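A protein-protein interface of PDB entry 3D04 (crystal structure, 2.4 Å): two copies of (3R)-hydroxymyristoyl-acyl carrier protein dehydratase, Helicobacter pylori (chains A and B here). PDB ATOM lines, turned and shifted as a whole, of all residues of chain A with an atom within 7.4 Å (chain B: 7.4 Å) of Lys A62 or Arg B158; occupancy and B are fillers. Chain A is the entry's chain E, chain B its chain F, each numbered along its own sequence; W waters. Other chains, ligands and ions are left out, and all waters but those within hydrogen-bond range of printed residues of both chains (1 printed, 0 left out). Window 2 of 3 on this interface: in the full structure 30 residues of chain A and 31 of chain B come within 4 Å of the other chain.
His B23 touches Gly A57 (CA to O, 3.6 Å). Pro B22 touches Phe A59 (CG to CE2, 3.8 Å). Phe A59 touches His B23. CB of Phe A59 touches NH2 of Arg B158, 3.5 Å away. CD of Pro A60 touches O of Pro B22 (3.8 Å). CG of Arg B24 touches CG of Pro A60 (3.8 Å). CD of Lys A62 touches CD1 of Ile B98, at 3.7 Å. Lys A62 touches Arg B158. Ile B98 touches Ile A64. Tyr B100 touches Ile A64 (OH to CD1, 3.6 Å).
Lys A62 touches just these residues of chain B: Ile B98 and Arg B158. Arg B158 touches just these residues of chain A: Phe A59, Pro A60 and Lys A62. Of the printed residues of chain A, Ile B98 touches Lys A62 and Ile A64. Of the printed residues of chain A, Arg B24 touches Gly A57 and Pro A60. Of the printed residues of chain B, Pro A60 touches Pro B22 (3.8 Å), Arg B24 (3.8 Å) and Arg B158 (2.5 Å). Of the printed residues of chain A, Pro B22 touches Phe A59 and Pro A60. Printed residues of chain A within 4 Å of Tyr B100: Ile A64 (3.6 Å). His A58 touches none of the printed residues of chain B. Phe A50 touches none of the printed residues of chain B. The nearest residue of chain A that does not touch Arg B158 is Asn A61 (4.4 Å). The nearest printed residue of chain A that does not touch Arg B24 is His A58 (5.0 Å).
Printed residues of chain A that touch a printed residue of chain B: Gly A57, Phe A59, Pro A60, Lys A62 and Ile A64. Printed residues of chain B that touch a printed residue of chain A: Pro B22, His B23, Arg B24, Ile B98, Tyr B100 and Arg B158. Hydrophobic or aromatic side chains of chain B that line the printed part of chain A: Pro B22, His B23, Ile B98 and Tyr B100. Along chain B the printed residues that touch a printed residue of chain A span positions 22 to 158. Among the printed residues, 12 pairs touch across the chains. Among the printed residues, no Asp or Glu carboxylate lies within 4 Å of a Lys or Arg side-chain nitrogen of the other chain.
Water W1 lies within hydrogen-bond range of a ring nitrogen (NE2) of His A58 and a ring nitrogen (NE2) of His B23.
No position is printed for both chains. Of the 12 pairs that touch across the chains among the printed residues, none has its exchanged pair printed and touching as well.
A ring nitrogen (ND1) of His A58 lies within hydrogen-bond range of the backbone carbonyl oxygen of Ile A64, at 2.6 Å. N of Arg B158 lies within hydrogen-bond range of O of Thr B96. The backbone NH (N) of Ile B98 lies within hydrogen-bond range of the backbone carbonyl oxygen (O) of Ala B156.
O of Gly A57 lies within hydrogen-bond range of N of Arg B24, 3.0 Å away. O of Pro A60 sits at hydrogen-bond distance from NH2 of Arg B158 (2.5 Å).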
ATOM      1  N   PHE A  50       8.322  -2.234 -37.891  1.00  0.00           N
ATOM      2  CA  PHE A  50       7.006  -1.968 -37.309  1.00  0.00           C
ATOM      3  C   PHE A  50       5.900  -2.757 -38.035  1.00  0.00           C
ATOM      4  O   PHE A  50       4.891  -3.111 -37.433  1.00  0.00           O
ATOM      5  CB  PHE A  50       6.691  -0.464 -37.278  1.00  0.00           C
ATOM      6  CG  PHE A  50       5.360  -0.137 -36.645  1.00  0.00           C
ATOM      7  CD1 PHE A  50       5.219  -0.113 -35.257  1.00  0.00           C
ATOM      8  CD2 PHE A  50       4.239   0.122 -37.440  1.00  0.00           C
ATOM      9  CE1 PHE A  50       3.983   0.167 -34.665  1.00  0.00           C
ATOM     10  CE2 PHE A  50       2.994   0.416 -36.855  1.00  0.00           C
ATOM     11  CZ  PHE A  50       2.867   0.430 -35.465  1.00  0.00           C
ATOM     12  N   PHE A  55       3.382  -6.552 -33.243  1.00  0.00           N
ATOM     13  CA  PHE A  55       3.496  -5.216 -32.657  1.00  0.00           C
ATOM     14  C   PHE A  55       2.150  -4.568 -32.312  1.00  0.00           C
ATOM     15  O   PHE A  55       2.090  -3.658 -31.478  1.00  0.00           O
ATOM     16  CB  PHE A  55       4.365  -4.307 -33.534  1.00  0.00           C
ATOM     17  CG  PHE A  55       5.836  -4.663 -33.511  1.00  0.00           C
ATOM     18  CD1 PHE A  55       6.508  -4.985 -34.685  1.00  0.00           C
ATOM     19  CD2 PHE A  55       6.542  -4.684 -32.311  1.00  0.00           C
ATOM     20  CE1 PHE A  55       7.873  -5.316 -34.665  1.00  0.00           C
ATOM     21  CE2 PHE A  55       7.901  -5.006 -32.280  1.00  0.00           C
ATOM     22  CZ  PHE A  55       8.568  -5.325 -33.459  1.00  0.00           C
ATOM     23  N   GLY A  57       0.035  -6.020 -30.529  1.00  0.00           N
ATOM     24  CA  GLY A  57      -0.195  -6.425 -29.155  1.00  0.00           C
ATOM     25  C   GLY A  57       0.952  -6.273 -28.171  1.00  0.00           C
ATOM     26  O   GLY A  57       0.761  -6.438 -26.972  1.00  0.00           O
ATOM     27  N   HIS A  58       2.136  -5.937 -28.664  1.00  0.00           N
ATOM     28  CA  HIS A  58       3.339  -5.966 -27.835  1.00  0.00           C
ATOM     29  C   HIS A  58       4.287  -4.785 -28.104  1.00  0.00           C
ATOM     30  O   HIS A  58       5.302  -4.963 -28.782  1.00  0.00           O
ATOM     31  CB  HIS A  58       4.077  -7.292 -28.071  1.00  0.00           C
ATOM     32  CG  HIS A  58       4.988  -7.697 -26.952  1.00  0.00           C
ATOM     33  ND1 HIS A  58       6.266  -7.198 -26.811  1.00  0.00           N
ATOM     34  CD2 HIS A  58       4.811  -8.570 -25.931  1.00  0.00           C
ATOM     35  CE1 HIS A  58       6.832  -7.739 -25.746  1.00  0.00           C
ATOM     36  NE2 HIS A  58       5.972  -8.578 -25.198  1.00  0.00           N
ATOM     37  N   PHE A  59       3.977  -3.583 -27.609  1.00  0.00           N
ATOM     38  CA  PHE A  59       2.720  -3.237 -26.941  1.00  0.00           C
ATOM     39  C   PHE A  59       2.115  -2.053 -27.697  1.00  0.00           C
ATOM     40  O   PHE A  59       2.838  -1.366 -28.413  1.00  0.00           O
ATOM     41  CB  PHE A  59       2.971  -2.850 -25.476  1.00  0.00           C
ATOM     42  CG  PHE A  59       3.609  -3.940 -24.654  1.00  0.00           C
ATOM     43  CD1 PHE A  59       4.995  -3.983 -24.484  1.00  0.00           C
ATOM     44  CD2 PHE A  59       2.828  -4.920 -24.042  1.00  0.00           C
ATOM     45  CE1 PHE A  59       5.592  -4.991 -23.723  1.00  0.00           C
ATOM     46  CE2 PHE A  59       3.418  -5.924 -23.278  1.00  0.00           C
ATOM     47  CZ  PHE A  59       4.803  -5.961 -23.118  1.00  0.00           C
ATOM     48  N   PRO A  60       0.797  -1.800 -27.548  1.00  0.00           N
ATOM     49  CA  PRO A  60       0.237  -0.587 -28.180  1.00  0.00           C
ATOM     50  C   PRO A  60       0.994   0.689 -27.771  1.00  0.00           C
ATOM     51  O   PRO A  60       1.222   0.922 -26.584  1.00  0.00           O
ATOM     52  CB  PRO A  60      -1.207  -0.556 -27.661  1.00  0.00           C
ATOM     53  CG  PRO A  60      -1.532  -2.007 -27.379  1.00  0.00           C
ATOM     54  CD  PRO A  60      -0.241  -2.573 -26.831  1.00  0.00           C
ATOM     55  N   ASN A  61       1.409   1.477 -28.761  1.00  0.00           N
ATOM     56  CA  ASN A  61       2.199   2.713 -28.551  1.00  0.00           C
ATOM     57  C   ASN A  61       3.659   2.520 -28.118  1.00  0.00           C
ATOM     58  O   ASN A  61       4.423   3.496 -28.051  1.00  0.00           O
ATOM     59  CB  ASN A  61       1.474   3.693 -27.616  1.00  0.00           C
ATOM     60  CG  ASN A  61       0.119   4.089 -28.146  1.00  0.00           C
ATOM     61  OD1 ASN A  61       0.004   4.587 -29.266  1.00  0.00           O
ATOM     62  ND2 ASN A  61      -0.922   3.844 -27.358  1.00  0.00           N
ATOM     63  N   LYS A  62       4.044   1.275 -27.836  1.00  0.00           N
ATOM     64  CA  LYS A  62       5.428   0.957 -27.483  1.00  0.00           C
ATOM     65  C   LYS A  62       5.854  -0.402 -28.066  1.00  0.00           C
ATOM     66  O   LYS A  62       5.832  -1.422 -27.366  1.00  0.00           O
ATOM     67  CB  LYS A  62       5.615   1.021 -25.958  1.00  0.00           C
ATOM     68  CG  LYS A  62       7.054   0.845 -25.488  1.00  0.00           C
ATOM     69  CD  LYS A  62       7.266   1.376 -24.077  1.00  0.00           C
ATOM     70  CE  LYS A  62       7.826   2.797 -24.102  1.00  0.00           C
ATOM     71  NZ  LYS A  62       9.156   2.869 -24.783  1.00  0.00           N
ATOM     72  N   PRO A  63       6.221  -0.423 -29.367  1.00  0.00           N
ATOM     73  CA  PRO A  63       6.583  -1.685 -30.027  1.00  0.00           C
ATOM     74  C   PRO A  63       7.887  -2.300 -29.505  1.00  0.00           C
ATOM     75  O   PRO A  63       8.959  -1.723 -29.651  1.00  0.00           O
ATOM     76  CB  PRO A  63       6.691  -1.299 -31.507  1.00  0.00           C
ATOM     77  CG  PRO A  63       6.931   0.160 -31.518  1.00  0.00           C
ATOM     78  CD  PRO A  63       6.281   0.726 -30.296  1.00  0.00           C
ATOM     79  N   ILE A  64       7.770  -3.462 -28.873  1.00  0.00           N
ATOM     80  CA  ILE A  64       8.915  -4.187 -28.324  1.00  0.00           C
ATOM     81  C   ILE A  64       8.862  -5.622 -28.840  1.00  0.00           C
ATOM     82  O   ILE A  64       7.899  -6.340 -28.578  1.00  0.00           O
ATOM     83  CB  ILE A  64       8.907  -4.162 -26.765  1.00  0.00           C
ATOM     84  CG1 ILE A  64       9.127  -2.730 -26.252  1.00  0.00           C
ATOM     85  CG2 ILE A  64       9.969  -5.108 -26.190  1.00  0.00           C
ATOM     86  CD1 ILE A  64       8.646  -2.485 -24.839  1.00  0.00           C
ATOM     87  N   PHE A  65       9.881  -6.032 -29.589  1.00  0.00           N
ATOM     88  CA  PHE A  65       9.942  -7.397 -30.099  1.00  0.00           C
ATOM     89  C   PHE A  65      10.017  -8.398 -28.940  1.00  0.00           C
ATOM     90  O   PHE A  65      10.935  -8.323 -28.123  1.00  0.00           O
ATOM     91  CB  PHE A  65      11.109  -7.579 -31.084  1.00  0.00           C
ATOM     92  CG  PHE A  65      11.004  -8.829 -31.925  1.00  0.00           C
ATOM     93  CD1 PHE A  65      10.077  -8.913 -32.962  1.00  0.00           C
ATOM     94  CD2 PHE A  65      11.822  -9.932 -31.668  1.00  0.00           C
ATOM     95  CE1 PHE A  65       9.974 -10.075 -33.737  1.00  0.00           C
ATOM     96  CE2 PHE A  65      11.718 -11.096 -32.430  1.00  0.00           C
ATOM     97  CZ  PHE A  65      10.794 -11.168 -33.466  1.00  0.00           C
ATOM     98  N   THR A 114      13.640  -3.381 -30.903  1.00  0.00           N
ATOM     99  CA  THR A 114      12.599  -2.501 -31.440  1.00  0.00           C
ATOM    100  C   THR A 114      12.635  -2.440 -32.974  1.00  0.00           C
ATOM    101  O   THR A 114      13.646  -2.799 -33.570  1.00  0.00           O
ATOM    102  CB  THR A 114      12.734  -1.063 -30.857  1.00  0.00           C
ATOM    103  OG1 THR A 114      13.970  -0.478 -31.293  1.00  0.00           O
ATOM    104  CG2 THR A 114      12.674  -1.071 -29.329  1.00  0.00           C
ATOM    105  N   PRO A 115      11.525  -2.000 -33.615  1.00  0.00           N
ATOM    106  CA  PRO A 115      11.496  -1.757 -35.064  1.00  0.00           C
ATOM    107  C   PRO A 115      12.708  -0.960 -35.560  1.00  0.00           C
ATOM    108  O   PRO A 115      13.093   0.034 -34.942  1.00  0.00           O
ATOM    109  CB  PRO A 115      10.208  -0.946 -35.249  1.00  0.00           C
ATOM    110  CG  PRO A 115       9.318  -1.456 -34.197  1.00  0.00           C
ATOM    111  CD  PRO A 115      10.205  -1.730 -33.008  1.00  0.00           C
ATOM    112  N   PRO B  22      -0.941  -5.268 -20.091  1.00  0.00           N
ATOM    113  CA  PRO B  22      -0.842  -4.365 -21.248  1.00  0.00           C
ATOM    114  C   PRO B  22      -0.892  -5.096 -22.593  1.00  0.00           C
ATOM    115  O   PRO B  22      -1.105  -4.462 -23.625  1.00  0.00           O
ATOM    116  CB  PRO B  22       0.526  -3.713 -21.062  1.00  0.00           C
ATOM    117  CG  PRO B  22       1.335  -4.753 -20.321  1.00  0.00           C
ATOM    118  CD  PRO B  22       0.371  -5.498 -19.447  1.00  0.00           C
ATOM    119  N   HIS B  23      -0.697  -6.416 -22.570  1.00  0.00           N
ATOM    120  CA  HIS B  23      -0.650  -7.229 -23.789  1.00  0.00           C
ATOM    121  C   HIS B  23      -1.977  -7.184 -24.544  1.00  0.00           C
ATOM    122  O   HIS B  23      -3.042  -7.199 -23.936  1.00  0.00           O
ATOM    123  CB  HIS B  23      -0.288  -8.676 -23.453  1.00  0.00           C
ATOM    124  CG  HIS B  23       0.947  -8.816 -22.620  1.00  0.00           C
ATOM    125  ND1 HIS B  23       0.960  -8.577 -21.262  1.00  0.00           N
ATOM    126  CD2 HIS B  23       2.209  -9.187 -22.949  1.00  0.00           C
ATOM    127  CE1 HIS B  23       2.178  -8.783 -20.792  1.00  0.00           C
ATOM    128  NE2 HIS B  23       2.955  -9.155 -21.795  1.00  0.00           N
ATOM    129  N   ARG B  24      -1.901  -7.109 -25.870  1.00  0.00           N
ATOM    130  CA  ARG B  24      -3.089  -7.146 -26.714  1.00  0.00           C
ATOM    131  C   ARG B  24      -2.889  -8.160 -27.822  1.00  0.00           C
ATOM    132  O   ARG B  24      -1.848  -8.802 -27.880  1.00  0.00           O
ATOM    133  CB  ARG B  24      -3.400  -5.757 -27.298  1.00  0.00           C
ATOM    134  CG  ARG B  24      -3.926  -4.731 -26.283  1.00  0.00           C
ATOM    135  CD  ARG B  24      -5.184  -5.229 -25.596  1.00  0.00           C
ATOM    136  NE  ARG B  24      -5.713  -4.235 -24.671  1.00  0.00           N
ATOM    137  CZ  ARG B  24      -5.486  -4.205 -23.359  1.00  0.00           C
ATOM    138  NH1 ARG B  24      -6.036  -3.247 -22.633  1.00  0.00           N
ATOM    139  NH2 ARG B  24      -4.732  -5.126 -22.768  1.00  0.00           N
ATOM    140  N   ALA B  94      -2.260   0.159 -13.519  1.00  0.00           N
ATOM    141  CA  ALA B  94      -1.960  -0.813 -14.569  1.00  0.00           C
ATOM    142  C   ALA B  94      -1.763  -0.178 -15.947  1.00  0.00           C
ATOM    143  O   ALA B  94      -0.830  -0.548 -16.667  1.00  0.00           O
ATOM    144  CB  ALA B  94      -3.040  -1.892 -14.627  1.00  0.00           C
ATOM    145  N   LYS B  95      -2.617   0.790 -16.296  1.00  0.00           N
ATOM    146  CA  LYS B  95      -2.604   1.393 -17.639  1.00  0.00           C
ATOM    147  C   LYS B  95      -1.330   2.174 -17.995  1.00  0.00           C
ATOM    148  O   LYS B  95      -1.115   2.521 -19.162  1.00  0.00           O
ATOM    149  CB  LYS B  95      -3.874   2.223 -17.898  1.00  0.00           C
ATOM    150  CG  LYS B  95      -3.792   3.715 -17.553  1.00  0.00           C
ATOM    151  CD  LYS B  95      -5.181   4.339 -17.368  1.00  0.00           C
ATOM    152  CE  LYS B  95      -6.101   4.075 -18.564  1.00  0.00           C
ATOM    153  NZ  LYS B  95      -7.536   3.941 -18.148  1.00  0.00           N
ATOM    154  N   THR B  96      -0.487   2.441 -16.997  1.00  0.00           N
ATOM    155  CA  THR B  96       0.774   3.155 -17.225  1.00  0.00           C
ATOM    156  C   THR B  96       1.973   2.214 -17.383  1.00  0.00           C
ATOM    157  O   THR B  96       3.045   2.636 -17.835  1.00  0.00           O
ATOM    158  CB  THR B  96       1.084   4.152 -16.081  1.00  0.00           C
ATOM    159  OG1 THR B  96       1.257   3.437 -14.850  1.00  0.00           O
ATOM    160  CG2 THR B  96      -0.038   5.176 -15.929  1.00  0.00           C
ATOM    161  N   LYS B  97       1.791   0.946 -17.008  1.00  0.00           N
ATOM    162  CA  LYS B  97       2.898  -0.009 -16.931  1.00  0.00           C
ATOM    163  C   LYS B  97       2.980  -0.937 -18.138  1.00  0.00           C
ATOM    164  O   LYS B  97       1.995  -1.133 -18.848  1.00  0.00           O
ATOM    165  CB  LYS B  97       2.804  -0.855 -15.657  1.00  0.00           C
ATOM    166  CG  LYS B  97       2.443  -0.107 -14.383  1.00  0.00           C
ATOM    167  CD  LYS B  97       3.585   0.722 -13.861  1.00  0.00           C
ATOM    168  CE  LYS B  97       3.234   1.316 -12.514  1.00  0.00           C
ATOM    169  NZ  LYS B  97       4.333   2.182 -12.008  1.00  0.00           N
ATOM    170  N   ILE B  98       4.176  -1.483 -18.365  1.00  0.00           N
ATOM    171  CA  ILE B  98       4.402  -2.596 -19.294  1.00  0.00           C
ATOM    172  C   ILE B  98       5.215  -3.679 -18.575  1.00  0.00           C
ATOM    173  O   ILE B  98       5.579  -3.515 -17.407  1.00  0.00           O
ATOM    174  CB  ILE B  98       5.106  -2.161 -20.626  1.00  0.00           C
ATOM    175  CG1 ILE B  98       6.393  -1.373 -20.346  1.00  0.00           C
ATOM    176  CG2 ILE B  98       4.143  -1.377 -21.526  1.00  0.00           C
ATOM    177  CD1 ILE B  98       7.367  -1.341 -21.512  1.00  0.00           C
ATOM    178  N   TYR B 100       8.611  -6.359 -18.996  1.00  0.00           N
ATOM    179  CA  TYR B 100       9.791  -6.900 -19.662  1.00  0.00           C
ATOM    180  C   TYR B 100      10.169  -8.267 -19.094  1.00  0.00           C
ATOM    181  O   TYR B 100      10.190  -8.459 -17.873  1.00  0.00           O
ATOM    182  CB  TYR B 100      10.990  -5.972 -19.478  1.00  0.00           C
ATOM    183  CG  TYR B 100      10.936  -4.671 -20.239  1.00  0.00           C
ATOM    184  CD1 TYR B 100      10.610  -3.478 -19.590  1.00  0.00           C
ATOM    185  CD2 TYR B 100      11.247  -4.625 -21.604  1.00  0.00           C
ATOM    186  CE1 TYR B 100      10.572  -2.267 -20.286  1.00  0.00           C
ATOM    187  CE2 TYR B 100      11.214  -3.426 -22.311  1.00  0.00           C
ATOM    188  CZ  TYR B 100      10.874  -2.248 -21.648  1.00  0.00           C
ATOM    189  OH  TYR B 100      10.843  -1.049 -22.343  1.00  0.00           O
ATOM    190  N   ALA B 156       7.519  -2.066 -15.584  1.00  0.00           N
ATOM    191  CA  ALA B 156       8.103  -0.741 -15.813  1.00  0.00           C
ATOM    192  C   ALA B 156       7.071   0.288 -16.270  1.00  0.00           C
ATOM    193  O   ALA B 156       6.043  -0.070 -16.846  1.00  0.00           O
ATOM    194  CB  ALA B 156       9.249  -0.831 -16.824  1.00  0.00           C
ATOM    195  N   GLU B 157       7.356   1.564 -15.999  1.00  0.00           N
ATOM    196  CA  GLU B 157       6.566   2.680 -16.517  1.00  0.00           C
ATOM    197  C   GLU B 157       6.707   2.775 -18.035  1.00  0.00           C
ATOM    198  O   GLU B 157       7.813   2.665 -18.565  1.00  0.00           O
ATOM    199  CB  GLU B 157       7.006   3.995 -15.868  1.00  0.00           C
ATOM    200  CG  GLU B 157       6.335   4.298 -14.538  1.00  0.00           C
ATOM    201  CD  GLU B 157       4.863   4.688 -14.686  1.00  0.00           C
ATOM    202  OE1 GLU B 157       4.021   4.104 -13.965  1.00  0.00           O
ATOM    203  OE2 GLU B 157       4.548   5.570 -15.522  1.00  0.00           O
ATOM    204  N   ARG B 158       5.585   2.977 -18.724  1.00  0.00           N
ATOM    205  CA  ARG B 158       5.563   3.013 -20.189  1.00  0.00           C
ATOM    206  C   ARG B 158       6.311   4.232 -20.744  1.00  0.00           C
ATOM    207  O   ARG B 158       6.419   5.266 -20.076  1.00  0.00           O
ATOM    208  CB  ARG B 158       4.122   2.994 -20.710  1.00  0.00           C
ATOM    209  CG  ARG B 158       3.994   2.316 -22.072  1.00  0.00           C
ATOM    210  CD  ARG B 158       2.771   2.813 -22.848  1.00  0.00           C
ATOM    211  NE  ARG B 158       2.282   1.792 -23.779  1.00  0.00           N
ATOM    212  CZ  ARG B 158       1.502   0.769 -23.420  1.00  0.00           C
ATOM    213  NH1 ARG B 158       1.125   0.628 -22.152  1.00  0.00           N
ATOM    214  NH2 ARG B 158       1.094  -0.114 -24.322  1.00  0.00           N
HETATM  215  O   HOH W   1       5.809 -10.038 -22.943  1.00  0.00           O
